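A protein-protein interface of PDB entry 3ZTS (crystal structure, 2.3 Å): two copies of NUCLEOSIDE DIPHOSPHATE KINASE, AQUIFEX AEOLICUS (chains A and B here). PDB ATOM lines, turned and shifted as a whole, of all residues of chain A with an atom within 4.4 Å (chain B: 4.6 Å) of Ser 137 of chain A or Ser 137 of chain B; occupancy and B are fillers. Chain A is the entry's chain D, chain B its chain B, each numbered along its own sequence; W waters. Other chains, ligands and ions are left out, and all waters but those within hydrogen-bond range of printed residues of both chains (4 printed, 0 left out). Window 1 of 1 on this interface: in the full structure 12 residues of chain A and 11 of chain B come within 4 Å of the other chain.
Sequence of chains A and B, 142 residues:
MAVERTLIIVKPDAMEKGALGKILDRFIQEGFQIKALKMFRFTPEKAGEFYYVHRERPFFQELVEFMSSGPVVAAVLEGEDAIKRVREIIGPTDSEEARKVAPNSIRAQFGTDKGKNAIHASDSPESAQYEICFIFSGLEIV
Phe 134 of chain A touches Ser 137 of chain B, and with the chains exchanged Ser 137 of chain A touches Phe 134 of chain B. Phe 134 of chain A touches Leu 139 of chain B, and with the chains exchanged Leu 139 of chain A touches Phe 134 of chain B. Ile 135 of chain A touches Leu 139 of chain B, and with the chains exchanged Leu 139 of chain A touches Ile 135 of chain B. Ser 137 of chain B touches its own counterpart, Ser 137 of chain A. Positions printed for both chains: 133, 134, 135, 136, 137, 138, 139, 140 and 141. Of the 18 pairs that touch across the chains among the printed residues, 18 have their exchanged pair printed and touching as well.
Water W1 lies within hydrogen-bond range of O of Phe 136 of chain B (2.5 Å), O of Cys 133 of chain A (3.3 Å), N of Gly 138 of chain B (3.3 Å) and SG of Cys 133 of chain B (3.8 Å). Water W4 lies within hydrogen-bond range of the backbone carbonyl oxygen of Phe 136 of chain A, the backbone carbonyl oxygen of Cys 133 of chain B, the backbone NH of Gly 138 of chain A and the side-chain sulfur of Cys 133 of chain A. Water W3 lies within hydrogen-bond range of the side-chain hydroxyl of Ser 137 of chain A, the side-chain carboxylate of Glu 140 of chain B and the side-chain carboxylate of Glu 140 of chain A. Water W2 lies within hydrogen-bond range of the side-chain carboxylate (OE1) of Glu 140 of chain A, the side-chain hydroxyl (OG) of Ser 137 of chain B and the side-chain carboxylate (OE2) of Glu 140 of chain B.
Among the printed residues, merely in contact across the chains: Ser 137 of chain A with Cys 133 of chain B (3.2 Å), Cys 133 of chain A with Ser 137 of chain B (3.3 Å), Ile 135 of chain A with Ser 137 of chain B (3.3 Å), Ser 137 of chain A with Ile 135 of chain B (3.4 Å), Phe 134 of chain A with Ser 137 of chain B (3.6 Å), Ser 137 of chain A with Phe 134 of chain B (3.6 Å), Ser 137 of chain A with Phe 136 of chain B (3.7 Å), Phe 136 of chain A with Ser 137 of chain B (3.7 Å), Leu 139 of chain A with Ile 135 of chain B (3.7 Å), Ser 137 of chain A with Ser 137 of chain B (3.8 Å) and Ile 135 of chain A with Leu 139 of chain B (3.8 Å).
Of the 9 printed residues of chain A, 7 touch a printed residue of chain B. Of the 9 printed residues of chain B, 7 touch a printed residue of chain A. Among the printed residues, 18 pairs touch across the chains.
Printed residues of chain B within 4 Å of Ser 137 of chain A: Cys 133 (3.2 Å), Phe 134 (3.6 Å), Ile 135 (3.4 Å), Phe 136 (3.7 Å) and Ser 137 (3.8 Å). Of the printed residues of chain A, Ser 137 of chain B touches Cys 133, Phe 134, Ile 135, Phe 136 and Ser 137. Of the printed residues of chain A, Cys 133 of chain B touches Cys 133 (3.2 Å), Ser 137 (3.2 Å) and Gly 138 (3.0 Å). Of the printed residues of chain A, Phe 136 of chain B touches Ser 137 (3.7 Å). Printed residues of chain A within 4 Å of Gly 138 of chain B: Cys 133 (3.0 Å) and Phe 134 (2.9 Å). Printed residues of chain B within 4 Å of Ile 135 of chain A: Ser 137 and Leu 139. Ile 141 of chain B touches none of the printed residues of chain A. Glu 140 of chain B touches none of the printed residues of chain A. The nearest printed residue of chain B that does not touch Ser 137 of chain A is Glu 140 of chain B (4.1 Å). The nearest printed residue of chain A that does not touch Ser 137 of chain B is Glu 140 of chain A (4.2 Å). The nearest printed residue of chain B that does not touch Phe 136 of chain A is Cys 133 of chain B (4.4 Å).
N of Gly 138 of chain A lies within hydrogen-bond range of O of Cys 133 of chain B, 3.0 Å away. The backbone carbonyl oxygen of Phe 134 of chain B sits at hydrogen-bond distance from the backbone NH of Gly 138 of chain A, 2.9 Å away. The backbone carbonyl oxygen (O) of Phe 134 of chain B is in hydrogen-bond range of the backbone NH (N) of Leu 139 of chain A. The backbone NH of Gly 138 of chain B is in hydrogen-bond range of the backbone carbonyl oxygen of Cys 133 of chain A (3.0 Å). The backbone NH of Gly 138 of chain B is in hydrogen-bond range of the backbone carbonyl oxygen of Phe 134 of chain A, 2.9 Å away. The backbone NH (N) of Leu 139 of chain B lies within hydrogen-bond range of the backbone carbonyl oxygen (O) of Phe 134 of chain A, at 3.0 Å. SG of Cys 133 of chain B lies close to SG of Cys 133 of chain A (3.2 Å).
OG of Ser 137 of chain B lies close to N of Leu 139 of chain B. N of Ser 137 of chain B is in hydrogen-bond range of OE2 of Glu 140 of chain B (2.9 Å). The side-chain hydroxyl (OG) of Ser 137 of chain A lies close to the backbone NH (N) of Leu 139 of chain A (3.1 Å). The backbone NH (N) of Ser 137 of chain A lies within hydrogen-bond range of the side-chain carboxylate (OE1) of Glu 140 of chain A, at 2.9 Å.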
ATOM      1  N   CYS A 133      20.808 -12.148  -6.357  1.00  0.00           N
ATOM      2  CA  CYS A 133      22.019 -11.897  -5.586  1.00  0.00           C
ATOM      3  C   CYS A 133      23.136 -11.291  -6.434  1.00  0.00           C
ATOM      4  O   CYS A 133      23.957 -10.510  -5.931  1.00  0.00           O
ATOM      5  CB  CYS A 133      22.500 -13.190  -4.915  1.00  0.00           C
ATOM      6  SG  CYS A 133      21.478 -13.695  -3.514  1.00  0.00           S
ATOM      7  N   PHE A 134      23.175 -11.646  -7.713  1.00  0.00           N
ATOM      8  CA  PHE A 134      24.196 -11.075  -8.579  1.00  0.00           C
ATOM      9  C   PHE A 134      24.033  -9.555  -8.706  1.00  0.00           C
ATOM     10  O   PHE A 134      25.016  -8.817  -8.750  1.00  0.00           O
ATOM     11  CB  PHE A 134      24.196 -11.736  -9.967  1.00  0.00           C
ATOM     12  CG  PHE A 134      25.478 -11.536 -10.711  1.00  0.00           C
ATOM     13  CD1 PHE A 134      25.685 -10.390 -11.459  1.00  0.00           C
ATOM     14  CD2 PHE A 134      26.499 -12.468 -10.621  1.00  0.00           C
ATOM     15  CE1 PHE A 134      26.889 -10.183 -12.128  1.00  0.00           C
ATOM     16  CE2 PHE A 134      27.703 -12.271 -11.285  1.00  0.00           C
ATOM     17  CZ  PHE A 134      27.899 -11.129 -12.039  1.00  0.00           C
ATOM     18  N   ILE A 135      22.786  -9.094  -8.745  1.00  0.00           N
ATOM     19  CA  ILE A 135      22.498  -7.686  -9.002  1.00  0.00           C
ATOM     20  C   ILE A 135      22.236  -6.872  -7.730  1.00  0.00           C
ATOM     21  O   ILE A 135      22.684  -5.735  -7.608  1.00  0.00           O
ATOM     22  CB  ILE A 135      21.288  -7.530  -9.958  1.00  0.00           C
ATOM     23  CG1 ILE A 135      21.535  -8.279 -11.273  1.00  0.00           C
ATOM     24  CG2 ILE A 135      21.026  -6.068 -10.236  1.00  0.00           C
ATOM     25  CD1 ILE A 135      22.791  -7.838 -11.986  1.00  0.00           C
ATOM     26  N   PHE A 136      21.504  -7.456  -6.788  1.00  0.00           N
ATOM     27  CA  PHE A 136      21.083  -6.749  -5.577  1.00  0.00           C
ATOM     28  C   PHE A 136      21.524  -7.465  -4.299  1.00  0.00           C
ATOM     29  O   PHE A 136      21.394  -8.684  -4.194  1.00  0.00           O
ATOM     30  CB  PHE A 136      19.559  -6.653  -5.536  1.00  0.00           C
ATOM     31  CG  PHE A 136      18.965  -5.811  -6.625  1.00  0.00           C
ATOM     32  CD1 PHE A 136      19.048  -4.427  -6.573  1.00  0.00           C
ATOM     33  CD2 PHE A 136      18.287  -6.401  -7.686  1.00  0.00           C
ATOM     34  CE1 PHE A 136      18.473  -3.640  -7.576  1.00  0.00           C
ATOM     35  CE2 PHE A 136      17.717  -5.628  -8.678  1.00  0.00           C
ATOM     36  CZ  PHE A 136      17.807  -4.246  -8.622  1.00  0.00           C
ATOM     37  N   SER A 137      22.029  -6.703  -3.330  1.00  0.00           N
ATOM     38  CA  SER A 137      22.294  -7.230  -1.997  1.00  0.00           C
ATOM     39  C   SER A 137      21.010  -7.204  -1.180  1.00  0.00           C
ATOM     40  O   SER A 137      20.044  -6.538  -1.549  1.00  0.00           O
ATOM     41  CB  SER A 137      23.346  -6.381  -1.286  1.00  0.00           C
ATOM     42  OG  SER A 137      22.801  -5.148  -0.841  1.00  0.00           O
ATOM     43  N   GLY A 138      21.003  -7.917  -0.064  1.00  0.00           N
ATOM     44  CA  GLY A 138      19.894  -7.834   0.862  1.00  0.00           C
ATOM     45  C   GLY A 138      19.655  -6.411   1.339  1.00  0.00           C
ATOM     46  O   GLY A 138      18.527  -6.022   1.632  1.00  0.00           O
ATOM     47  N   LEU A 139      20.720  -5.624   1.421  1.00  0.00           N
ATOM     48  CA  LEU A 139      20.602  -4.226   1.814  1.00  0.00           C
ATOM     49  C   LEU A 139      19.790  -3.387   0.811  1.00  0.00           C
ATOM     50  O   LEU A 139      19.194  -2.372   1.179  1.00  0.00           O
ATOM     51  CB  LEU A 139      21.990  -3.611   1.995  1.00  0.00           C
ATOM     52  CG  LEU A 139      22.825  -4.206   3.130  1.00  0.00           C
ATOM     53  CD1 LEU A 139      24.230  -3.581   3.139  1.00  0.00           C
ATOM     54  CD2 LEU A 139      22.108  -4.026   4.480  1.00  0.00           C
ATOM     55  N   GLU A 140      19.771  -3.807  -0.452  1.00  0.00           N
ATOM     56  CA  GLU A 140      19.057  -3.072  -1.499  1.00  0.00           C
ATOM     57  C   GLU A 140      17.605  -3.534  -1.684  1.00  0.00           C
ATOM     58  O   GLU A 140      16.859  -2.946  -2.462  1.00  0.00           O
ATOM     59  CB  GLU A 140      19.777  -3.191  -2.839  1.00  0.00           C
ATOM     60  CG  GLU A 140      21.146  -2.530  -2.907  1.00  0.00           C
ATOM     61  CD  GLU A 140      21.910  -2.937  -4.168  1.00  0.00           C
ATOM     62  OE1 GLU A 140      22.614  -3.967  -4.128  1.00  0.00           O
ATOM     63  OE2 GLU A 140      21.797  -2.241  -5.203  1.00  0.00           O
ATOM     64  N   ILE A 141      17.210  -4.595  -0.994  1.00  0.00           N
ATOM     65  CA  ILE A 141      15.845  -5.086  -1.111  1.00  0.00           C
ATOM     66  C   ILE A 141      15.047  -4.449  -0.001  1.00  0.00           C
ATOM     67  O   ILE A 141      15.296  -4.715   1.171  1.00  0.00           O
ATOM     68  CB  ILE A 141      15.759  -6.597  -0.920  1.00  0.00           C
ATOM     69  CG1 ILE A 141      16.935  -7.290  -1.607  1.00  0.00           C
ATOM     70  CG2 ILE A 141      14.429  -7.112  -1.425  1.00  0.00           C
ATOM     71  CD1 ILE A 141      16.689  -7.655  -3.001  1.00  0.00           C
ATOM     72  N   CYS B 133      25.588 -12.410   0.380  1.00  0.00           N
ATOM     73  CA  CYS B 133      24.524 -11.876  -0.473  1.00  0.00           C
ATOM     74  C   CYS B 133      23.709 -10.796   0.225  1.00  0.00           C
ATOM     75  O   CYS B 133      23.223  -9.864  -0.417  1.00  0.00           O
ATOM     76  CB  CYS B 133      23.600 -12.995  -0.981  1.00  0.00           C
ATOM     77  SG  CYS B 133      24.371 -14.057  -2.231  1.00  0.00           S
ATOM     78  N   PHE B 134      23.560 -10.916   1.540  1.00  0.00           N
ATOM     79  CA  PHE B 134      22.837  -9.900   2.287  1.00  0.00           C
ATOM     80  C   PHE B 134      23.525  -8.538   2.189  1.00  0.00           C
ATOM     81  O   PHE B 134      22.863  -7.508   2.102  1.00  0.00           O
ATOM     82  CB  PHE B 134      22.669 -10.299   3.763  1.00  0.00           C
ATOM     83  CG  PHE B 134      21.544  -9.577   4.440  1.00  0.00           C
ATOM     84  CD1 PHE B 134      20.255 -10.085   4.396  1.00  0.00           C
ATOM     85  CD2 PHE B 134      21.762  -8.365   5.065  1.00  0.00           C
ATOM     86  CE1 PHE B 134      19.213  -9.404   4.988  1.00  0.00           C
ATOM     87  CE2 PHE B 134      20.718  -7.677   5.661  1.00  0.00           C
ATOM     88  CZ  PHE B 134      19.442  -8.196   5.621  1.00  0.00           C
ATOM     89  N   ILE B 135      24.853  -8.539   2.208  1.00  0.00           N
ATOM     90  CA  ILE B 135      25.628  -7.295   2.253  1.00  0.00           C
ATOM     91  C   ILE B 135      26.101  -6.810   0.876  1.00  0.00           C
ATOM     92  O   ILE B 135      26.084  -5.620   0.600  1.00  0.00           O
ATOM     93  CB  ILE B 135      26.869  -7.433   3.187  1.00  0.00           C
ATOM     94  CG1 ILE B 135      26.452  -7.841   4.612  1.00  0.00           C
ATOM     95  CG2 ILE B 135      27.689  -6.142   3.203  1.00  0.00           C
ATOM     96  CD1 ILE B 135      25.417  -6.932   5.237  1.00  0.00           C
ATOM     97  N   PHE B 136      26.521  -7.740   0.026  1.00  0.00           N
ATOM     98  CA  PHE B 136      27.148  -7.408  -1.252  1.00  0.00           C
ATOM     99  C   PHE B 136      26.463  -8.122  -2.420  1.00  0.00           C
ATOM    100  O   PHE B 136      26.173  -9.316  -2.338  1.00  0.00           O
ATOM    101  CB  PHE B 136      28.613  -7.851  -1.253  1.00  0.00           C
ATOM    102  CG  PHE B 136      29.496  -7.118  -0.275  1.00  0.00           C
ATOM    103  CD1 PHE B 136      29.947  -5.830  -0.550  1.00  0.00           C
ATOM    104  CD2 PHE B 136      29.931  -7.740   0.886  1.00  0.00           C
ATOM    105  CE1 PHE B 136      30.788  -5.162   0.331  1.00  0.00           C
ATOM    106  CE2 PHE B 136      30.777  -7.081   1.770  1.00  0.00           C
ATOM    107  CZ  PHE B 136      31.205  -5.791   1.495  1.00  0.00           C
ATOM    108  N   SER B 137      26.220  -7.396  -3.508  1.00  0.00           N
ATOM    109  CA  SER B 137      25.761  -8.023  -4.744  1.00  0.00           C
ATOM    110  C   SER B 137      26.961  -8.557  -5.518  1.00  0.00           C
ATOM    111  O   SER B 137      28.105  -8.226  -5.213  1.00  0.00           O
ATOM    112  CB  SER B 137      24.999  -7.029  -5.626  1.00  0.00           C
ATOM    113  OG  SER B 137      25.888  -6.117  -6.241  1.00  0.00           O
ATOM    114  N   GLY B 138      26.699  -9.386  -6.518  1.00  0.00           N
ATOM    115  CA  GLY B 138      27.752  -9.832  -7.407  1.00  0.00           C
ATOM    116  C   GLY B 138      28.464  -8.668  -8.086  1.00  0.00           C
ATOM    117  O   GLY B 138      29.656  -8.760  -8.379  1.00  0.00           O
ATOM    118  N   LEU B 139      27.737  -7.577  -8.326  1.00  0.00           N
ATOM    119  CA  LEU B 139      28.304  -6.371  -8.929  1.00  0.00           C
ATOM    120  C   LEU B 139      29.369  -5.714  -8.047  1.00  0.00           C
ATOM    121  O   LEU B 139      30.246  -5.019  -8.555  1.00  0.00           O
ATOM    122  CB  LEU B 139      27.195  -5.356  -9.224  1.00  0.00           C
ATOM    123  CG  LEU B 139      26.152  -5.826 -10.235  1.00  0.00           C
ATOM    124  CD1 LEU B 139      25.069  -4.749 -10.418  1.00  0.00           C
ATOM    125  CD2 LEU B 139      26.843  -6.182 -11.554  1.00  0.00           C
ATOM    126  N   GLU B 140      29.281  -5.937  -6.735  1.00  0.00           N
ATOM    127  CA  GLU B 140      30.217  -5.348  -5.773  1.00  0.00           C
ATOM    128  C   GLU B 140      31.441  -6.224  -5.489  1.00  0.00           C
ATOM    129  O   GLU B 140      32.366  -5.803  -4.791  1.00  0.00           O
ATOM    130  CB  GLU B 140      29.509  -5.042  -4.448  1.00  0.00           C
ATOM    131  CG  GLU B 140      28.387  -4.019  -4.550  1.00  0.00           C
ATOM    132  CD  GLU B 140      27.652  -3.842  -3.224  1.00  0.00           C
ATOM    133  OE1 GLU B 140      28.082  -2.999  -2.413  1.00  0.00           O
ATOM    134  OE2 GLU B 140      26.647  -4.550  -2.990  1.00  0.00           O
ATOM    135  N   ILE B 141      31.432  -7.449  -5.998  1.00  0.00           N
ATOM    136  CA  ILE B 141      32.542  -8.366  -5.766  1.00  0.00           C
ATOM    137  C   ILE B 141      33.490  -8.208  -6.932  1.00  0.00           C
ATOM    138  O   ILE B 141      33.133  -8.525  -8.059  1.00  0.00           O
ATOM    139  CB  ILE B 141      32.062  -9.823  -5.741  1.00  0.00           C
ATOM    140  CG1 ILE B 141      30.769  -9.952  -4.934  1.00  0.00           C
ATOM    141  CG2 ILE B 141      33.132 -10.736  -5.188  1.00  0.00           C
ATOM    142  CD1 ILE B 141      30.975 -10.099  -3.479  1.00  0.00           C
HETATM  143  O   HOH W   1      26.378 -11.290  -3.866  1.00  0.00           O
HETATM  144  O   HOH W   2      24.960  -3.611  -5.494  1.00  0.00           O
HETATM  145  O   HOH W   3      24.531  -3.317  -1.736  1.00  0.00           O
HETATM  146  O   HOH W   4      20.600 -10.366  -2.384  1.00  0.00           O
